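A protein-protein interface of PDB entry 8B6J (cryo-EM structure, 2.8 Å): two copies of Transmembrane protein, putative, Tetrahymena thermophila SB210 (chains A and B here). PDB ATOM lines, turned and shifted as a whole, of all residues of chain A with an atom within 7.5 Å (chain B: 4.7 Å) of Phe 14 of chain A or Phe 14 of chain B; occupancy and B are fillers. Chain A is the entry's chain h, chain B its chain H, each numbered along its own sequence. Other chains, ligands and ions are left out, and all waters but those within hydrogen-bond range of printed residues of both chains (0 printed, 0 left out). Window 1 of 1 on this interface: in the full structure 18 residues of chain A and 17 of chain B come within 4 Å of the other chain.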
ATOM      1  N   VAL A  11      14.620   0.382  -9.018  1.00  0.00           N
ATOM      2  CA  VAL A  11      15.153   0.211  -7.672  1.00  0.00           C
ATOM      3  C   VAL A  11      14.123  -0.534  -6.836  1.00  0.00           C
ATOM      4  O   VAL A  11      12.962  -0.116  -6.752  1.00  0.00           O
ATOM      5  CB  VAL A  11      15.502   1.564  -7.031  1.00  0.00           C
ATOM      6  CG1 VAL A  11      16.021   1.365  -5.618  1.00  0.00           C
ATOM      7  CG2 VAL A  11      16.524   2.303  -7.880  1.00  0.00           C
ATOM      8  N   LYS A  12      14.548  -1.634  -6.217  1.00  0.00           N
ATOM      9  CA  LYS A  12      13.698  -2.385  -5.296  1.00  0.00           C
ATOM     10  C   LYS A  12      13.771  -1.691  -3.945  1.00  0.00           C
ATOM     11  O   LYS A  12      14.663  -1.944  -3.134  1.00  0.00           O
ATOM     12  CB  LYS A  12      14.139  -3.841  -5.212  1.00  0.00           C
ATOM     13  CG  LYS A  12      13.976  -4.607  -6.513  1.00  0.00           C
ATOM     14  CD  LYS A  12      14.370  -6.065  -6.356  1.00  0.00           C
ATOM     15  CE  LYS A  12      14.181  -6.832  -7.656  1.00  0.00           C
ATOM     16  NZ  LYS A  12      14.570  -8.263  -7.525  1.00  0.00           N
ATOM     17  N   ASP A  13      12.810  -0.808  -3.701  1.00  0.00           N
ATOM     18  CA  ASP A  13      12.828   0.090  -2.561  1.00  0.00           C
ATOM     19  C   ASP A  13      11.656  -0.217  -1.637  1.00  0.00           C
ATOM     20  O   ASP A  13      10.634  -0.762  -2.057  1.00  0.00           O
ATOM     21  CB  ASP A  13      12.764   1.549  -3.024  1.00  0.00           C
ATOM     22  CG  ASP A  13      13.459   2.490  -2.074  1.00  0.00           C
ATOM     23  OD1 ASP A  13      13.534   2.164  -0.873  1.00  0.00           O
ATOM     24  OD2 ASP A  13      13.933   3.550  -2.531  1.00  0.00           O
ATOM     25  N   PHE A  14      11.818   0.140  -0.365  1.00  0.00           N
ATOM     26  CA  PHE A  14      10.786  -0.128   0.628  1.00  0.00           C
ATOM     27  C   PHE A  14      11.042   0.726   1.859  1.00  0.00           C
ATOM     28  O   PHE A  14      12.155   0.729   2.391  1.00  0.00           O
ATOM     29  CB  PHE A  14      10.765  -1.613   0.999  1.00  0.00           C
ATOM     30  CG  PHE A  14       9.712  -1.971   2.001  1.00  0.00           C
ATOM     31  CD1 PHE A  14       8.393  -2.122   1.615  1.00  0.00           C
ATOM     32  CD2 PHE A  14      10.040  -2.165   3.328  1.00  0.00           C
ATOM     33  CE1 PHE A  14       7.422  -2.452   2.535  1.00  0.00           C
ATOM     34  CE2 PHE A  14       9.076  -2.494   4.251  1.00  0.00           C
ATOM     35  CZ  PHE A  14       7.765  -2.640   3.855  1.00  0.00           C
ATOM     36  N   HIS A  15      10.014   1.441   2.307  1.00  0.00           N
ATOM     37  CA  HIS A  15      10.098   2.281   3.500  1.00  0.00           C
ATOM     38  C   HIS A  15       9.620   1.463   4.692  1.00  0.00           C
ATOM     39  O   HIS A  15       8.416   1.317   4.916  1.00  0.00           O
ATOM     40  CB  HIS A  15       9.270   3.548   3.327  1.00  0.00           C
ATOM     41  CG  HIS A  15       9.740   4.429   2.212  1.00  0.00           C
ATOM     42  ND1 HIS A  15      10.458   5.585   2.430  1.00  0.00           N
ATOM     43  CD2 HIS A  15       9.598   4.321   0.870  1.00  0.00           C
ATOM     44  CE1 HIS A  15      10.736   6.153   1.270  1.00  0.00           C
ATOM     45  NE2 HIS A  15      10.226   5.405   0.308  1.00  0.00           N
ATOM     46  N   SER A  16      10.564   0.928   5.460  1.00  0.00           N
ATOM     47  CA  SER A  16      10.208   0.118   6.614  1.00  0.00           C
ATOM     48  C   SER A  16       9.454   0.952   7.641  1.00  0.00           C
ATOM     49  O   SER A  16       9.753   2.131   7.849  1.00  0.00           O
ATOM     50  CB  SER A  16      11.463  -0.479   7.249  1.00  0.00           C
ATOM     51  OG  SER A  16      11.133  -1.256   8.386  1.00  0.00           O
ATOM     52  N   ASP A  17       8.468   0.330   8.285  1.00  0.00           N
ATOM     53  CA  ASP A  17       7.728   0.992   9.350  1.00  0.00           C
ATOM     54  C   ASP A  17       8.487   1.006  10.668  1.00  0.00           C
ATOM     55  O   ASP A  17       8.014   1.623  11.627  1.00  0.00           O
ATOM     56  CB  ASP A  17       6.369   0.319   9.547  1.00  0.00           C
ATOM     57  CG  ASP A  17       5.348   0.754   8.512  1.00  0.00           C
ATOM     58  OD1 ASP A  17       5.709   1.542   7.615  1.00  0.00           O
ATOM     59  OD2 ASP A  17       4.184   0.311   8.600  1.00  0.00           O
ATOM     60  N   GLU A  18       9.637   0.343  10.742  1.00  0.00           N
ATOM     61  CA  GLU A  18      10.489   0.474  11.913  1.00  0.00           C
ATOM     62  C   GLU A  18      10.956   1.917  12.046  1.00  0.00           C
ATOM     63  O   GLU A  18      11.151   2.623  11.054  1.00  0.00           O
ATOM     64  CB  GLU A  18      11.691  -0.466  11.805  1.00  0.00           C
ATOM     65  CG  GLU A  18      12.581  -0.487  13.034  1.00  0.00           C
ATOM     66  CD  GLU A  18      13.847  -1.291  12.820  1.00  0.00           C
ATOM     67  OE1 GLU A  18      14.004  -1.873  11.725  1.00  0.00           O
ATOM     68  OE2 GLU A  18      14.688  -1.340  13.742  1.00  0.00           O
ATOM     69  N   GLN A  33       4.088  -5.437  12.654  1.00  0.00           N
ATOM     70  CA  GLN A  33       4.261  -4.994  11.275  1.00  0.00           C
ATOM     71  C   GLN A  33       5.636  -5.381  10.747  1.00  0.00           C
ATOM     72  O   GLN A  33       5.771  -5.811   9.595  1.00  0.00           O
ATOM     73  CB  GLN A  33       4.057  -3.481  11.185  1.00  0.00           C
ATOM     74  CG  GLN A  33       4.208  -2.903   9.786  1.00  0.00           C
ATOM     75  CD  GLN A  33       3.155  -3.411   8.826  1.00  0.00           C
ATOM     76  OE1 GLN A  33       2.095  -3.876   9.240  1.00  0.00           O
ATOM     77  NE2 GLN A  33       3.441  -3.325   7.534  1.00  0.00           N
ATOM     78  N   GLY A  34       6.670  -5.248  11.580  1.00  0.00           N
ATOM     79  CA  GLY A  34       8.022  -5.539  11.141  1.00  0.00           C
ATOM     80  C   GLY A  34       8.213  -6.954  10.637  1.00  0.00           C
ATOM     81  O   GLY A  34       9.126  -7.202   9.843  1.00  0.00           O
ATOM     82  N   ASN A  35       7.376  -7.892  11.082  1.00  0.00           N
ATOM     83  CA  ASN A  35       7.490  -9.267  10.616  1.00  0.00           C
ATOM     84  C   ASN A  35       7.180  -9.405   9.133  1.00  0.00           C
ATOM     85  O   ASN A  35       7.543 -10.421   8.530  1.00  0.00           O
ATOM     86  CB  ASN A  35       6.564 -10.172  11.426  1.00  0.00           C
ATOM     87  CG  ASN A  35       7.019 -10.332  12.859  1.00  0.00           C
ATOM     88  OD1 ASN A  35       7.820  -9.544  13.358  1.00  0.00           O
ATOM     89  ND2 ASN A  35       6.514 -11.359  13.528  1.00  0.00           N
ATOM     90  N   LEU A  36       6.530  -8.417   8.529  1.00  0.00           N
ATOM     91  CA  LEU A  36       6.205  -8.484   7.108  1.00  0.00           C
ATOM     92  C   LEU A  36       7.419  -8.298   6.212  1.00  0.00           C
ATOM     93  O   LEU A  36       7.244  -8.210   4.991  1.00  0.00           O
ATOM     94  CB  LEU A  36       5.140  -7.441   6.769  1.00  0.00           C
ATOM     95  CG  LEU A  36       3.693  -7.830   7.079  1.00  0.00           C
ATOM     96  CD1 LEU A  36       3.544  -8.321   8.505  1.00  0.00           C
ATOM     97  CD2 LEU A  36       2.774  -6.651   6.830  1.00  0.00           C
ATOM     98  N   ILE A  37       8.627  -8.226   6.759  1.00  0.00           N
ATOM     99  CA  ILE A  37       9.851  -8.162   5.963  1.00  0.00           C
ATOM    100  C   ILE A  37      10.388  -9.589   5.915  1.00  0.00           C
ATOM    101  O   ILE A  37      11.132 -10.029   6.791  1.00  0.00           O
ATOM    102  CB  ILE A  37      10.863  -7.181   6.548  1.00  0.00           C
ATOM    103  CG1 ILE A  37      10.174  -5.884   6.973  1.00  0.00           C
ATOM    104  CG2 ILE A  37      11.958  -6.889   5.538  1.00  0.00           C
ATOM    105  CD1 ILE A  37       9.362  -5.232   5.885  1.00  0.00           C
ATOM    106  N   TYR A  38      10.008 -10.318   4.870  1.00  0.00           N
ATOM    107  CA  TYR A  38      10.358 -11.728   4.769  1.00  0.00           C
ATOM    108  C   TYR A  38      11.854 -11.908   4.553  1.00  0.00           C
ATOM    109  O   TYR A  38      12.531 -11.054   3.977  1.00  0.00           O
ATOM    110  CB  TYR A  38       9.602 -12.384   3.617  1.00  0.00           C
ATOM    111  CG  TYR A  38       8.106 -12.204   3.674  1.00  0.00           C
ATOM    112  CD1 TYR A  38       7.450 -12.030   4.883  1.00  0.00           C
ATOM    113  CD2 TYR A  38       7.349 -12.206   2.515  1.00  0.00           C
ATOM    114  CE1 TYR A  38       6.085 -11.865   4.935  1.00  0.00           C
ATOM    115  CE2 TYR A  38       5.986 -12.046   2.556  1.00  0.00           C
ATOM    116  CZ  TYR A  38       5.358 -11.873   3.768  1.00  0.00           C
ATOM    117  OH  TYR A  38       3.995 -11.708   3.807  1.00  0.00           O
ATOM    118  N   GLY A  39      12.366 -13.043   5.022  1.00  0.00           N
ATOM    119  CA  GLY A  39      13.730 -13.426   4.724  1.00  0.00           C
ATOM    120  C   GLY A  39      14.794 -12.662   5.473  1.00  0.00           C
ATOM    121  O   GLY A  39      15.942 -12.630   5.026  1.00  0.00           O
ATOM    122  N   SER A  40      14.452 -12.046   6.599  1.00  0.00           N
ATOM    123  CA  SER A  40      15.409 -11.312   7.415  1.00  0.00           C
ATOM    124  C   SER A  40      15.477 -11.948   8.795  1.00  0.00           C
ATOM    125  O   SER A  40      14.443 -12.179   9.428  1.00  0.00           O
ATOM    126  CB  SER A  40      15.022  -9.835   7.530  1.00  0.00           C
ATOM    127  OG  SER A  40      13.755  -9.686   8.145  1.00  0.00           O
ATOM    128  N   TYR A  47      13.861 -17.913  11.375  1.00  0.00           N
ATOM    129  CA  TYR A  47      14.486 -18.039  10.066  1.00  0.00           C
ATOM    130  C   TYR A  47      15.786 -18.830  10.096  1.00  0.00           C
ATOM    131  O   TYR A  47      16.320 -19.145   9.029  1.00  0.00           O
ATOM    132  CB  TYR A  47      14.744 -16.652   9.476  1.00  0.00           C
ATOM    133  CG  TYR A  47      13.506 -16.003   8.905  1.00  0.00           C
ATOM    134  CD1 TYR A  47      13.019 -16.374   7.662  1.00  0.00           C
ATOM    135  CD2 TYR A  47      12.825 -15.022   9.608  1.00  0.00           C
ATOM    136  CE1 TYR A  47      11.887 -15.787   7.136  1.00  0.00           C
ATOM    137  CE2 TYR A  47      11.693 -14.428   9.089  1.00  0.00           C
ATOM    138  CZ  TYR A  47      11.229 -14.815   7.853  1.00  0.00           C
ATOM    139  OH  TYR A  47      10.102 -14.228   7.331  1.00  0.00           O
ATOM    140  N   LYS B  12       1.228  -4.310   3.483  1.00  0.00           N
ATOM    141  CA  LYS B  12       2.504  -3.729   3.072  1.00  0.00           C
ATOM    142  C   LYS B  12       3.581  -4.790   3.239  1.00  0.00           C
ATOM    143  O   LYS B  12       4.127  -4.982   4.326  1.00  0.00           O
ATOM    144  CB  LYS B  12       2.820  -2.482   3.889  1.00  0.00           C
ATOM    145  CG  LYS B  12       1.996  -1.269   3.495  1.00  0.00           C
ATOM    146  CD  LYS B  12       2.484  -0.015   4.199  1.00  0.00           C
ATOM    147  CE  LYS B  12       1.698   1.209   3.763  1.00  0.00           C
ATOM    148  NZ  LYS B  12       2.206   2.454   4.402  1.00  0.00           N
ATOM    149  N   ASP B  13       3.894  -5.480   2.148  1.00  0.00           N
ATOM    150  CA  ASP B  13       4.731  -6.666   2.173  1.00  0.00           C
ATOM    151  C   ASP B  13       6.007  -6.420   1.383  1.00  0.00           C
ATOM    152  O   ASP B  13       6.009  -5.688   0.389  1.00  0.00           O
ATOM    153  CB  ASP B  13       3.975  -7.861   1.590  1.00  0.00           C
ATOM    154  CG  ASP B  13       4.592  -9.181   1.971  1.00  0.00           C
ATOM    155  OD1 ASP B  13       5.828  -9.237   2.133  1.00  0.00           O
ATOM    156  OD2 ASP B  13       3.834 -10.163   2.111  1.00  0.00           O
ATOM    157  N   PHE B  14       7.097  -7.037   1.834  1.00  0.00           N
ATOM    158  CA  PHE B  14       8.377  -6.906   1.156  1.00  0.00           C
ATOM    159  C   PHE B  14       9.181  -8.182   1.345  1.00  0.00           C
ATOM    160  O   PHE B  14       9.178  -8.770   2.429  1.00  0.00           O
ATOM    161  CB  PHE B  14       9.165  -5.704   1.682  1.00  0.00           C
ATOM    162  CG  PHE B  14      10.395  -5.389   0.883  1.00  0.00           C
ATOM    163  CD1 PHE B  14      10.293  -4.805  -0.366  1.00  0.00           C
ATOM    164  CD2 PHE B  14      11.652  -5.673   1.382  1.00  0.00           C
ATOM    165  CE1 PHE B  14      11.421  -4.514  -1.103  1.00  0.00           C
ATOM    166  CE2 PHE B  14      12.783  -5.384   0.648  1.00  0.00           C
ATOM    167  CZ  PHE B  14      12.668  -4.803  -0.594  1.00  0.00           C
ATOM    168  N   HIS B  15       9.869  -8.601   0.285  1.00  0.00           N
ATOM    169  CA  HIS B  15      10.735  -9.779   0.310  1.00  0.00           C
ATOM    170  C   HIS B  15      12.175  -9.288   0.394  1.00  0.00           C
ATOM    171  O   HIS B  15      12.773  -8.910  -0.615  1.00  0.00           O
ATOM    172  CB  HIS B  15      10.512 -10.645  -0.925  1.00  0.00           C
ATOM    173  CG  HIS B  15       9.095 -11.092  -1.103  1.00  0.00           C
ATOM    174  ND1 HIS B  15       8.628 -12.293  -0.616  1.00  0.00           N
ATOM    175  CD2 HIS B  15       8.044 -10.499  -1.715  1.00  0.00           C
ATOM    176  CE1 HIS B  15       7.349 -12.420  -0.920  1.00  0.00           C
ATOM    177  NE2 HIS B  15       6.970 -11.344  -1.587  1.00  0.00           N
ATOM    178  N   SER B  16      12.731  -9.298   1.602  1.00  0.00           N
ATOM    179  CA  SER B  16      14.078  -8.784   1.802  1.00  0.00           C
ATOM    180  C   SER B  16      15.088  -9.608   1.016  1.00  0.00           C
ATOM    181  O   SER B  16      15.030 -10.840   0.991  1.00  0.00           O
ATOM    182  CB  SER B  16      14.438  -8.800   3.286  1.00  0.00           C
ATOM    183  OG  SER B  16      15.737  -8.277   3.498  1.00  0.00           O
ATOM    184  N   LEU B  36      18.758  -0.492   1.026  1.00  0.00           N
ATOM    185  CA  LEU B  36      17.550   0.053   0.419  1.00  0.00           C
ATOM    186  C   LEU B  36      16.330  -0.077   1.318  1.00  0.00           C
ATOM    187  O   LEU B  36      15.267   0.444   0.966  1.00  0.00           O
ATOM    188  CB  LEU B  36      17.283  -0.626  -0.924  1.00  0.00           C
ATOM    189  CG  LEU B  36      18.037  -0.018  -2.108  1.00  0.00           C
ATOM    190  CD1 LEU B  36      19.539  -0.071  -1.885  1.00  0.00           C
ATOM    191  CD2 LEU B  36      17.663  -0.722  -3.402  1.00  0.00           C
ATOM    192  N   ILE B  37      16.447  -0.763   2.453  1.00  0.00           N
ATOM    193  CA  ILE B  37      15.375  -0.812   3.445  1.00  0.00           C
ATOM    194  C   ILE B  37      15.473   0.472   4.262  1.00  0.00           C
ATOM    195  O   ILE B  37      16.245   0.555   5.218  1.00  0.00           O
ATOM    196  CB  ILE B  37      15.473  -2.053   4.335  1.00  0.00           C
ATOM    197  CG1 ILE B  37      15.747  -3.303   3.496  1.00  0.00           C
ATOM    198  CG2 ILE B  37      14.197  -2.227   5.142  1.00  0.00           C
ATOM    199  CD1 ILE B  37      14.759  -3.526   2.380  1.00  0.00           C
ATOM    200  N   TYR B  38      14.694   1.481   3.886  1.00  0.00           N
ATOM    201  CA  TYR B  38      14.756   2.761   4.571  1.00  0.00           C
ATOM    202  C   TYR B  38      14.109   2.668   5.947  1.00  0.00           C
ATOM    203  O   TYR B  38      13.270   1.806   6.214  1.00  0.00           O
ATOM    204  CB  TYR B  38      14.061   3.847   3.752  1.00  0.00           C
ATOM    205  CG  TYR B  38      14.591   4.004   2.348  1.00  0.00           C
ATOM    206  CD1 TYR B  38      15.867   3.579   2.011  1.00  0.00           C
ATOM    207  CD2 TYR B  38      13.813   4.584   1.361  1.00  0.00           C
ATOM    208  CE1 TYR B  38      16.351   3.725   0.729  1.00  0.00           C
ATOM    209  CE2 TYR B  38      14.287   4.738   0.080  1.00  0.00           C
ATOM    210  CZ  TYR B  38      15.555   4.304  -0.233  1.00  0.00           C
ATOM    211  OH  TYR B  38      16.027   4.453  -1.515  1.00  0.00           O
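The backbone NH (N) of Tyr 38 of chain B lies within hydrogen-bond range of the backbone carbonyl oxygen (O) of Phe 14 of chain A. The side-chain carboxylate of Asp 13 of chain B sits close to the backbone carbonyl oxygen of Leu 36 of chain A (3.4 Å). The side-chain carboxylate (OD2) of Asp 13 of chain B sits close to the side-chain hydroxyl (OH) of Tyr 38 of chain A, 2.3 Å away. N of Ser 16 of chain A sits at hydrogen-bond distance from O of Tyr 38 of chain B (2.9 Å). The backbone NH of Phe 14 of chain B lies within hydrogen-bond range of the backbone carbonyl oxygen of Leu 36 of chain A, 3.4 Å away. O of Leu 36 of chain B lies close to OD1 of Asp 13 of chain A (3.1 Å). OH of Tyr 38 of chain B sits at hydrogen-bond distance from OD2 of Asp 13 of chain A (2.5 Å). The backbone NH (N) of Ser 16 of chain B lies within hydrogen-bond range of the backbone carbonyl oxygen (O) of Tyr 38 of chain A (3.0 Å). The backbone NH (N) of Tyr 38 of chain A is in hydrogen-bond range of the backbone carbonyl oxygen (O) of Phe 14 of chain B, 3.0 Å away. The backbone carbonyl oxygen (O) of Phe 14 of chain A sits close to the backbone carbonyl oxygen (O) of Leu 36 of chain B (3.4 Å).
OG of Ser 40 of chain A sits at hydrogen-bond distance from O of Ile 37 of chain A. The side-chain hydroxyl (OG) of Ser 16 of chain A lies close to the backbone NH (N) of Glu 18 of chain A, 3.2 Å away.
Among the printed residues, pairs that only touch across the chains: Val 11 of chain A with Leu 36 of chain B (3.5 Å), Lys 12 of chain A with Leu 36 of chain B (3.3 Å), Asp 13 of chain A with Phe 14 of chain B (3.95 Å), Phe 14 of chain A with Phe 14 of chain B (3.5 Å), Phe 14 of chain A with Ile 37 of chain B (3.7 Å), His 15 of chain A with Tyr 38 of chain B (3.5 Å), Ser 16 of chain A with Ile 37 of chain B (3.9 Å), Gln 33 of chain A with Lys 12 of chain B (3.7 Å), Leu 36 of chain A with Lys 12 of chain B (3.3 Å), Ile 37 of chain A with Phe 14 of chain B (3.6 Å), Ile 37 of chain A with Ser 16 of chain B (3.9 Å) and Tyr 38 of chain A with His 15 of chain B (3.4 Å).
Glu 18 of chain A touches none of the printed residues of chain B. Printed residues of chain B within 4 Å of Tyr 38 of chain A: Asp 13 (2.3 Å), Phe 14 (3.0 Å), His 15 (3.4 Å) and Ser 16 (3.0 Å). Tyr 47 of chain A touches none of the printed residues of chain B. Printed residues of chain A within 4 Å of Lys 12 of chain B: Gln 33 and Leu 36. Phe 14 of chain B touches just these residues of chain A: Asp 13 (3.95 Å), Phe 14 (3.5 Å), Leu 36 (3.3 Å), Ile 37 (3.6 Å) and Tyr 38 (3.0 Å). The nearest printed residue of chain A that does not touch Lys 12 of chain B is Phe 14 of chain A (4.4 Å).
Of the 8 printed residues of chain B, 8 touch a printed residue of chain A. Hydrophobic or aromatic side chains of chain B within 4 Å of the printed part of chain A: Phe 14, His 15, Leu 36, Ile 37 and Tyr 38. Of the 17 printed residues of chain A, 10 touch a printed residue of chain B. Hydrophobic or aromatic side chains of chain A that line the printed part of chain B: Val 11, Phe 14, His 15, Leu 36, Ile 37 and Tyr 38. Among the printed residues, no Asp or Glu carboxylate lies within 4 Å of a Lys or Arg side-chain nitrogen of the other chain.
Lys 12 of chain A touches Leu 36 of chain B, and with the chains exchanged Leu 36 of chain A touches Lys 12 of chain B. Asp 13 of chain A touches Phe 14 of chain B, but with the chains exchanged Phe 14 of chain A does not touch Asp 13 of chain B (4.1 Å). Phe 14 of chain B touches its own counterpart, Phe 14 of chain A. Phe 14 of chain A touches Ile 37 of chain B, and with the chains exchanged Ile 37 of chain A touches Phe 14 of chain B. Positions printed for both chains: 12, 13, 14, 15, 16, 36, 37 and 38. Of the 22 pairs that touch across the chains among the printed residues, 19 have their exchanged pair printed and touching as well.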
